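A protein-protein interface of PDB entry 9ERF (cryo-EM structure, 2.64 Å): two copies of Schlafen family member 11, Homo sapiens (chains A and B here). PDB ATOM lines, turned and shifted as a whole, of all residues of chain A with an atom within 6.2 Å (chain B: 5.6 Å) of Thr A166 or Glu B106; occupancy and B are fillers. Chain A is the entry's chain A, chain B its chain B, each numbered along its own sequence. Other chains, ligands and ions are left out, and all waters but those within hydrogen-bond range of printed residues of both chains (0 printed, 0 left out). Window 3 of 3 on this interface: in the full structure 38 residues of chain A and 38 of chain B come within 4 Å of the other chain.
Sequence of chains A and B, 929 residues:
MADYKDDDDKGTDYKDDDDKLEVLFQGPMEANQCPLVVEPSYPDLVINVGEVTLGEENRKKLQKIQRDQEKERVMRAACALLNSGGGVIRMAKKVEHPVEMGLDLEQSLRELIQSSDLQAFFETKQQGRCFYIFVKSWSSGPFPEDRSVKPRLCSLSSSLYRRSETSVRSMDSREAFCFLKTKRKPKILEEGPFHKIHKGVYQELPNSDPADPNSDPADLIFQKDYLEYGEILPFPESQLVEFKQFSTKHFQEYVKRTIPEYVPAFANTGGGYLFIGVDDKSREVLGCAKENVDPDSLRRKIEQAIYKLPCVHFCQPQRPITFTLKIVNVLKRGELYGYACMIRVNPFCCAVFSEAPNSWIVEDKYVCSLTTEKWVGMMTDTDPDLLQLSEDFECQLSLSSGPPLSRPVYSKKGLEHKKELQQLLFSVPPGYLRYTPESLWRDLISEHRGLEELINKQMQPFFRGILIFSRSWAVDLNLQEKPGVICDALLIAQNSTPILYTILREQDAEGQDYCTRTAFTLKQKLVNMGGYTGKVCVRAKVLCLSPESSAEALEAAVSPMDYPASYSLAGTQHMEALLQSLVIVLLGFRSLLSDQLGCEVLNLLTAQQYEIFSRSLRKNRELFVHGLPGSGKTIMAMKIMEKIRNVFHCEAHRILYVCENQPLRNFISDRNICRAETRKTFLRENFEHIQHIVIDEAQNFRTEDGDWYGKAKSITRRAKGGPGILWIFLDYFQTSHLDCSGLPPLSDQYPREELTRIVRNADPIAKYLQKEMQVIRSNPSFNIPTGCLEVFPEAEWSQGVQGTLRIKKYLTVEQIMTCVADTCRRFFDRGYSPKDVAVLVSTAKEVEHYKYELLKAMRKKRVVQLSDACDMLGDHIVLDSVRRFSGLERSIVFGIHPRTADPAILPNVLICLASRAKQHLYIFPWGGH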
ATOM      1  N   ARG A 163      23.242 -17.010  -9.733  1.00  0.00           N
ATOM      2  CA  ARG A 163      23.592 -18.416  -9.632  1.00  0.00           C
ATOM      3  C   ARG A 163      22.834 -19.192 -10.702  1.00  0.00           C
ATOM      4  O   ARG A 163      21.604 -19.120 -10.774  1.00  0.00           O
ATOM      5  CB  ARG A 163      23.256 -18.926  -8.233  1.00  0.00           C
ATOM      6  CG  ARG A 163      23.757 -20.312  -7.925  1.00  0.00           C
ATOM      7  CD  ARG A 163      25.253 -20.367  -7.781  1.00  0.00           C
ATOM      8  NE  ARG A 163      25.674 -21.675  -7.301  1.00  0.00           N
ATOM      9  CZ  ARG A 163      26.924 -22.000  -7.008  1.00  0.00           C
ATOM     10  NH1 ARG A 163      27.908 -21.126  -7.114  1.00  0.00           N
ATOM     11  NH2 ARG A 163      27.192 -23.236  -6.604  1.00  0.00           N
ATOM     12  N   SER A 164      23.569 -19.909 -11.550  1.00  0.00           N
ATOM     13  CA  SER A 164      22.993 -20.749 -12.601  1.00  0.00           C
ATOM     14  C   SER A 164      23.483 -22.163 -12.334  1.00  0.00           C
ATOM     15  O   SER A 164      24.555 -22.556 -12.793  1.00  0.00           O
ATOM     16  CB  SER A 164      23.386 -20.266 -13.981  1.00  0.00           C
ATOM     17  OG  SER A 164      23.011 -18.918 -14.164  1.00  0.00           O
ATOM     18  N   GLU A 165      22.688 -22.927 -11.591  1.00  0.00           N
ATOM     19  CA  GLU A 165      23.128 -24.221 -11.091  1.00  0.00           C
ATOM     20  C   GLU A 165      24.384 -24.017 -10.254  1.00  0.00           C
ATOM     21  O   GLU A 165      24.352 -23.275  -9.269  1.00  0.00           O
ATOM     22  CB  GLU A 165      23.371 -25.201 -12.243  1.00  0.00           C
ATOM     23  CG  GLU A 165      22.114 -25.621 -12.978  1.00  0.00           C
ATOM     24  CD  GLU A 165      21.050 -26.170 -12.053  1.00  0.00           C
ATOM     25  OE1 GLU A 165      19.942 -25.594 -12.012  1.00  0.00           O
ATOM     26  OE2 GLU A 165      21.318 -27.178 -11.369  1.00  0.00           O
ATOM     27  N   THR A 166      25.492 -24.639 -10.634  1.00  0.00           N
ATOM     28  CA  THR A 166      26.700 -24.616  -9.823  1.00  0.00           C
ATOM     29  C   THR A 166      27.663 -23.502 -10.209  1.00  0.00           C
ATOM     30  O   THR A 166      28.803 -23.509  -9.738  1.00  0.00           O
ATOM     31  CB  THR A 166      27.424 -25.961  -9.922  1.00  0.00           C
ATOM     32  OG1 THR A 166      27.928 -26.137 -11.251  1.00  0.00           O
ATOM     33  CG2 THR A 166      26.483 -27.098  -9.595  1.00  0.00           C
ATOM     34  N   SER A 167      27.252 -22.551 -11.042  1.00  0.00           N
ATOM     35  CA  SER A 167      28.165 -21.541 -11.550  1.00  0.00           C
ATOM     36  C   SER A 167      27.561 -20.159 -11.363  1.00  0.00           C
ATOM     37  O   SER A 167      26.345 -19.995 -11.262  1.00  0.00           O
ATOM     38  CB  SER A 167      28.495 -21.776 -13.027  1.00  0.00           C
ATOM     39  OG  SER A 167      27.363 -21.548 -13.837  1.00  0.00           O
ATOM     40  N   VAL A 168      28.438 -19.164 -11.314  1.00  0.00           N
ATOM     41  CA  VAL A 168      28.054 -17.764 -11.200  1.00  0.00           C
ATOM     42  C   VAL A 168      28.256 -17.112 -12.557  1.00  0.00           C
ATOM     43  O   VAL A 168      29.355 -17.166 -13.121  1.00  0.00           O
ATOM     44  CB  VAL A 168      28.876 -17.051 -10.112  1.00  0.00           C
ATOM     45  CG1 VAL A 168      28.524 -15.577 -10.060  1.00  0.00           C
ATOM     46  CG2 VAL A 168      28.649 -17.712  -8.765  1.00  0.00           C
ATOM     47  N   GLU A 237      27.686 -29.598  -4.928  1.00  0.00           N
ATOM     48  CA  GLU A 237      27.379 -28.220  -5.277  1.00  0.00           C
ATOM     49  C   GLU A 237      26.131 -28.185  -6.147  1.00  0.00           C
ATOM     50  O   GLU A 237      25.871 -29.099  -6.931  1.00  0.00           O
ATOM     51  CB  GLU A 237      28.549 -27.579  -6.019  1.00  0.00           C
ATOM     52  CG  GLU A 237      29.764 -27.321  -5.161  1.00  0.00           C
ATOM     53  CD  GLU A 237      30.869 -26.638  -5.928  1.00  0.00           C
ATOM     54  OE1 GLU A 237      31.005 -26.918  -7.133  1.00  0.00           O
ATOM     55  OE2 GLU A 237      31.604 -25.827  -5.332  1.00  0.00           O
ATOM     56  N   SER A 238      25.349 -27.126  -6.003  1.00  0.00           N
ATOM     57  CA  SER A 238      24.077 -27.035  -6.705  1.00  0.00           C
ATOM     58  C   SER A 238      23.678 -25.568  -6.797  1.00  0.00           C
ATOM     59  O   SER A 238      24.490 -24.668  -6.561  1.00  0.00           O
ATOM     60  CB  SER A 238      23.013 -27.884  -6.000  1.00  0.00           C
ATOM     61  OG  SER A 238      22.654 -27.332  -4.748  1.00  0.00           O
ATOM     62  N   GLN A 239      22.415 -25.331  -7.152  1.00  0.00           N
ATOM     63  CA  GLN A 239      21.893 -23.974  -7.222  1.00  0.00           C
ATOM     64  C   GLN A 239      21.985 -23.268  -5.877  1.00  0.00           C
ATOM     65  O   GLN A 239      21.988 -22.034  -5.823  1.00  0.00           O
ATOM     66  CB  GLN A 239      20.442 -24.019  -7.708  1.00  0.00           C
ATOM     67  CG  GLN A 239      19.718 -22.688  -7.764  1.00  0.00           C
ATOM     68  CD  GLN A 239      20.134 -21.843  -8.941  1.00  0.00           C
ATOM     69  OE1 GLN A 239      20.198 -22.320 -10.070  1.00  0.00           O
ATOM     70  NE2 GLN A 239      20.409 -20.576  -8.686  1.00  0.00           N
ATOM     71  N   VAL A 241      24.296 -24.422  -3.190  1.00  0.00           N
ATOM     72  CA  VAL A 241      25.491 -24.787  -2.437  1.00  0.00           C
ATOM     73  C   VAL A 241      26.723 -24.477  -3.273  1.00  0.00           C
ATOM     74  O   VAL A 241      26.723 -24.675  -4.490  1.00  0.00           O
ATOM     75  CB  VAL A 241      25.482 -26.273  -2.031  1.00  0.00           C
ATOM     76  CG1 VAL A 241      26.802 -26.654  -1.405  1.00  0.00           C
ATOM     77  CG2 VAL A 241      24.343 -26.557  -1.071  1.00  0.00           C
ATOM     78  N   GLU A 242      27.768 -23.984  -2.615  1.00  0.00           N
ATOM     79  CA  GLU A 242      29.065 -23.742  -3.228  1.00  0.00           C
ATOM     80  C   GLU A 242      30.160 -24.173  -2.261  1.00  0.00           C
ATOM     81  O   GLU A 242      30.105 -23.853  -1.072  1.00  0.00           O
ATOM     82  CB  GLU A 242      29.226 -22.261  -3.592  1.00  0.00           C
ATOM     83  CG  GLU A 242      30.571 -21.899  -4.188  1.00  0.00           C
ATOM     84  CD  GLU A 242      30.790 -22.521  -5.542  1.00  0.00           C
ATOM     85  OE1 GLU A 242      29.793 -22.797  -6.235  1.00  0.00           O
ATOM     86  OE2 GLU A 242      31.958 -22.742  -5.916  1.00  0.00           O
ATOM     87  N   TYR A 262      30.315 -14.510  -4.972  1.00  0.00           N
ATOM     88  CA  TYR A 262      29.294 -15.501  -4.664  1.00  0.00           C
ATOM     89  C   TYR A 262      28.120 -14.947  -3.870  1.00  0.00           C
ATOM     90  O   TYR A 262      26.979 -15.339  -4.127  1.00  0.00           O
ATOM     91  CB  TYR A 262      29.928 -16.674  -3.915  1.00  0.00           C
ATOM     92  CG  TYR A 262      30.846 -17.475  -4.802  1.00  0.00           C
ATOM     93  CD1 TYR A 262      30.339 -18.437  -5.658  1.00  0.00           C
ATOM     94  CD2 TYR A 262      32.211 -17.243  -4.815  1.00  0.00           C
ATOM     95  CE1 TYR A 262      31.161 -19.156  -6.482  1.00  0.00           C
ATOM     96  CE2 TYR A 262      33.041 -17.960  -5.638  1.00  0.00           C
ATOM     97  CZ  TYR A 262      32.510 -18.918  -6.469  1.00  0.00           C
ATOM     98  OH  TYR A 262      33.331 -19.643  -7.296  1.00  0.00           O
ATOM     99  N   GLU B 100      25.776 -33.457  -9.392  1.00  0.00           N
ATOM    100  CA  GLU B 100      25.511 -32.289 -10.213  1.00  0.00           C
ATOM    101  C   GLU B 100      25.498 -32.685 -11.686  1.00  0.00           C
ATOM    102  O   GLU B 100      26.092 -33.685 -12.096  1.00  0.00           O
ATOM    103  CB  GLU B 100      26.551 -31.196  -9.945  1.00  0.00           C
ATOM    104  CG  GLU B 100      27.932 -31.433 -10.549  1.00  0.00           C
ATOM    105  CD  GLU B 100      28.714 -32.513  -9.831  1.00  0.00           C
ATOM    106  OE1 GLU B 100      28.272 -32.948  -8.748  1.00  0.00           O
ATOM    107  OE2 GLU B 100      29.770 -32.928 -10.348  1.00  0.00           O
ATOM    108  N   MET B 101      24.797 -31.888 -12.489  1.00  0.00           N
ATOM    109  CA  MET B 101      24.637 -32.220 -13.900  1.00  0.00           C
ATOM    110  C   MET B 101      25.981 -32.236 -14.619  1.00  0.00           C
ATOM    111  O   MET B 101      26.331 -33.222 -15.276  1.00  0.00           O
ATOM    112  CB  MET B 101      23.692 -31.216 -14.555  1.00  0.00           C
ATOM    113  CG  MET B 101      22.861 -31.780 -15.687  1.00  0.00           C
ATOM    114  SD  MET B 101      21.544 -30.667 -16.215  1.00  0.00           S
ATOM    115  CE  MET B 101      22.253 -29.064 -15.849  1.00  0.00           C
ATOM    116  N   GLY B 102      26.752 -31.164 -14.495  1.00  0.00           N
ATOM    117  CA  GLY B 102      28.005 -31.026 -15.216  1.00  0.00           C
ATOM    118  C   GLY B 102      28.069 -29.693 -15.933  1.00  0.00           C
ATOM    119  O   GLY B 102      27.071 -29.191 -16.456  1.00  0.00           O
ATOM    120  N   LEU B 103      29.269 -29.113 -15.967  1.00  0.00           N
ATOM    121  CA  LEU B 103      29.429 -27.770 -16.512  1.00  0.00           C
ATOM    122  C   LEU B 103      29.113 -27.708 -18.000  1.00  0.00           C
ATOM    123  O   LEU B 103      28.507 -26.734 -18.454  1.00  0.00           O
ATOM    124  CB  LEU B 103      30.849 -27.269 -16.256  1.00  0.00           C
ATOM    125  CG  LEU B 103      31.221 -27.029 -14.795  1.00  0.00           C
ATOM    126  CD1 LEU B 103      32.668 -26.607 -14.688  1.00  0.00           C
ATOM    127  CD2 LEU B 103      30.317 -25.979 -14.179  1.00  0.00           C
ATOM    128  N   ASP B 104      29.529 -28.707 -18.780  1.00  0.00           N
ATOM    129  CA  ASP B 104      29.251 -28.667 -20.212  1.00  0.00           C
ATOM    130  C   ASP B 104      27.755 -28.740 -20.487  1.00  0.00           C
ATOM    131  O   ASP B 104      27.244 -28.028 -21.361  1.00  0.00           O
ATOM    132  CB  ASP B 104      29.994 -29.795 -20.930  1.00  0.00           C
ATOM    133  CG  ASP B 104      29.569 -31.167 -20.462  1.00  0.00           C
ATOM    134  OD1 ASP B 104      29.313 -31.330 -19.254  1.00  0.00           O
ATOM    135  OD2 ASP B 104      29.494 -32.084 -21.304  1.00  0.00           O
ATOM    136  N   LEU B 105      27.034 -29.583 -19.748  1.00  0.00           N
ATOM    137  CA  LEU B 105      25.585 -29.656 -19.907  1.00  0.00           C
ATOM    138  C   LEU B 105      24.925 -28.345 -19.492  1.00  0.00           C
ATOM    139  O   LEU B 105      24.022 -27.847 -20.178  1.00  0.00           O
ATOM    140  CB  LEU B 105      25.034 -30.824 -19.089  1.00  0.00           C
ATOM    141  CG  LEU B 105      25.544 -32.217 -19.475  1.00  0.00           C
ATOM    142  CD1 LEU B 105      25.153 -33.234 -18.425  1.00  0.00           C
ATOM    143  CD2 LEU B 105      25.030 -32.643 -20.834  1.00  0.00           C
ATOM    144  N   GLU B 106      25.370 -27.768 -18.373  1.00  0.00           N
ATOM    145  CA  GLU B 106      24.848 -26.476 -17.938  1.00  0.00           C
ATOM    146  C   GLU B 106      25.041 -25.422 -19.018  1.00  0.00           C
ATOM    147  O   GLU B 106      24.124 -24.655 -19.332  1.00  0.00           O
ATOM    148  CB  GLU B 106      25.550 -26.031 -16.656  1.00  0.00           C
ATOM    149  CG  GLU B 106      25.142 -26.754 -15.404  1.00  0.00           C
ATOM    150  CD  GLU B 106      25.909 -26.263 -14.191  1.00  0.00           C
ATOM    151  OE1 GLU B 106      26.590 -25.224 -14.296  1.00  0.00           O
ATOM    152  OE2 GLU B 106      25.839 -26.918 -13.134  1.00  0.00           O
ATOM    153  N   GLN B 107      26.244 -25.362 -19.587  1.00  0.00           N
ATOM    154  CA  GLN B 107      26.547 -24.329 -20.567  1.00  0.00           C
ATOM    155  C   GLN B 107      25.762 -24.548 -21.851  1.00  0.00           C
ATOM    156  O   GLN B 107      25.337 -23.584 -22.492  1.00  0.00           O
ATOM    157  CB  GLN B 107      28.047 -24.297 -20.853  1.00  0.00           C
ATOM    158  CG  GLN B 107      28.475 -23.150 -21.757  1.00  0.00           C
ATOM    159  CD  GLN B 107      28.066 -21.792 -21.212  1.00  0.00           C
ATOM    160  OE1 GLN B 107      28.121 -21.551 -20.008  1.00  0.00           O
ATOM    161  NE2 GLN B 107      27.630 -20.907 -22.097  1.00  0.00           N
ATOM    162  N   SER B 108      25.564 -25.804 -22.247  1.00  0.00           N
ATOM    163  CA  SER B 108      24.749 -26.073 -23.426  1.00  0.00           C
ATOM    164  C   SER B 108      23.303 -25.650 -23.205  1.00  0.00           C
ATOM    165  O   SER B 108      22.673 -25.092 -24.107  1.00  0.00           O
ATOM    166  CB  SER B 108      24.831 -27.549 -23.794  1.00  0.00           C
ATOM    167  OG  SER B 108      26.163 -27.916 -24.091  1.00  0.00           O
ATOM    168  N   LEU B 109      22.754 -25.903 -22.016  1.00  0.00           N
ATOM    169  CA  LEU B 109      21.395 -25.443 -21.735  1.00  0.00           C
ATOM    170  C   LEU B 109      21.318 -23.921 -21.742  1.00  0.00           C
ATOM    171  O   LEU B 109      20.343 -23.339 -22.244  1.00  0.00           O
ATOM    172  CB  LEU B 109      20.919 -25.997 -20.394  1.00  0.00           C
ATOM    173  CG  LEU B 109      20.740 -27.512 -20.314  1.00  0.00           C
ATOM    174  CD1 LEU B 109      20.461 -27.932 -18.894  1.00  0.00           C
ATOM    175  CD2 LEU B 109      19.630 -27.976 -21.229  1.00  0.00           C
ATOM    176  N   ARG B 110      22.330 -23.260 -21.178  1.00  0.00           N
ATOM    177  CA  ARG B 110      22.360 -21.803 -21.190  1.00  0.00           C
ATOM    178  C   ARG B 110      22.424 -21.267 -22.610  1.00  0.00           C
ATOM    179  O   ARG B 110      21.780 -20.268 -22.931  1.00  0.00           O
ATOM    180  CB  ARG B 110      23.548 -21.291 -20.383  1.00  0.00           C
ATOM    181  CG  ARG B 110      23.344 -21.330 -18.895  1.00  0.00           C
ATOM    182  CD  ARG B 110      24.516 -20.719 -18.171  1.00  0.00           C
ATOM    183  NE  ARG B 110      24.725 -21.356 -16.878  1.00  0.00           N
ATOM    184  CZ  ARG B 110      25.737 -22.158 -16.578  1.00  0.00           C
ATOM    185  NH1 ARG B 110      26.705 -22.410 -17.442  1.00  0.00           N
ATOM    186  NH2 ARG B 110      25.778 -22.724 -15.379  1.00  0.00           N
ATOM    187  N   GLU B 111      23.218 -21.904 -23.468  1.00  0.00           N
ATOM    188  CA  GLU B 111      23.258 -21.515 -24.873  1.00  0.00           C
ATOM    189  C   GLU B 111      21.915 -21.743 -25.546  1.00  0.00           C
ATOM    190  O   GLU B 111      21.493 -20.939 -26.383  1.00  0.00           O
ATOM    191  CB  GLU B 111      24.340 -22.305 -25.605  1.00  0.00           C
ATOM    192  CG  GLU B 111      25.746 -21.808 -25.369  1.00  0.00           C
ATOM    193  CD  GLU B 111      26.790 -22.887 -25.588  1.00  0.00           C
ATOM    194  OE1 GLU B 111      26.445 -23.952 -26.142  1.00  0.00           O
ATOM    195  OE2 GLU B 111      27.957 -22.671 -25.201  1.00  0.00           O
ATOM    196  N   LEU B 118      18.595 -20.482 -15.829  1.00  0.00           N
ATOM    197  CA  LEU B 118      18.296 -21.866 -16.172  1.00  0.00           C
ATOM    198  C   LEU B 118      17.032 -22.345 -15.471  1.00  0.00           C
ATOM    199  O   LEU B 118      16.251 -23.111 -16.040  1.00  0.00           O
ATOM    200  CB  LEU B 118      19.483 -22.752 -15.801  1.00  0.00           C
ATOM    201  CG  LEU B 118      20.577 -22.953 -16.852  1.00  0.00           C
ATOM    202  CD1 LEU B 118      21.633 -23.896 -16.313  1.00  0.00           C
ATOM    203  CD2 LEU B 118      20.025 -23.477 -18.157  1.00  0.00           C
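The backbone carbonyl oxygen of Ser A164 is in hydrogen-bond range of the guanidinium group of Arg B110 (2.9 Å).
The side-chain hydroxyl (OG1) of Thr A166 lies within hydrogen-bond range of the side-chain carboxylate (OE2) of Glu B106, at 2.9 Å.
The side-chain hydroxyl (OG) of Ser A167 lies within hydrogen-bond range of the guanidinium group (NH2) of Arg B110 (2.5 Å).
NE of Arg A163 lies within hydrogen-bond range of O of Glu A165, 2.9 Å away.
O of Ser A164 lies within hydrogen-bond range of OG of Ser A167, at 3.2 Å.
The backbone NH (N) of Glu A165 is in hydrogen-bond range of the side-chain amide oxygen (OE1) of Gln A239, at 3.0 Å.
OE1 of Glu B106 lies within salt-bridge range of NH2 of Arg B110 (2.8 Å).
NH1 of Arg B110 sits at hydrogen-bond distance from OE1 of Gln B107, 3.1 Å away.
Among the printed residues, pairs that only touch across the chains: Glu A165 with Glu B106, Ser A164 with Glu B106, Glu A237 with Glu B100, Thr A166 with Leu B103, Ser A167 with Glu B106 and Glu A165 with Leu B118.
Of the printed residues of chain B, Ser A164 touches Glu B106 (3.7 Å) and Arg B110 (2.9 Å).
Thr A166 touches two residues of chain B.
Glu B106 touches four residues of chain A.
Of the printed residues of chain A, Arg B110 touches Ser A164 and Ser A167.
Printed residues of chain A that touch a printed residue of chain B: Ser A164, Glu A165, Thr A166, Ser A167 and Glu A237.
Printed residues of chain B that touch a printed residue of chain A: Glu B100, Leu B103, Glu B106, Arg B110 and Leu B118.
Hydrophobic or aromatic side chains of chain B that line the printed part of chain A: Leu B103 and Leu B118.
Among the printed residues, 9 pairs touch across the chains.
Among the printed residues, no Asp or Glu carboxylate lies within 4 Å of a Lys or Arg side-chain nitrogen of the other chain.
No position is printed for both chains.
Of the 9 pairs that touch across the chains among the printed residues, none has its exchanged pair printed and touching as well.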
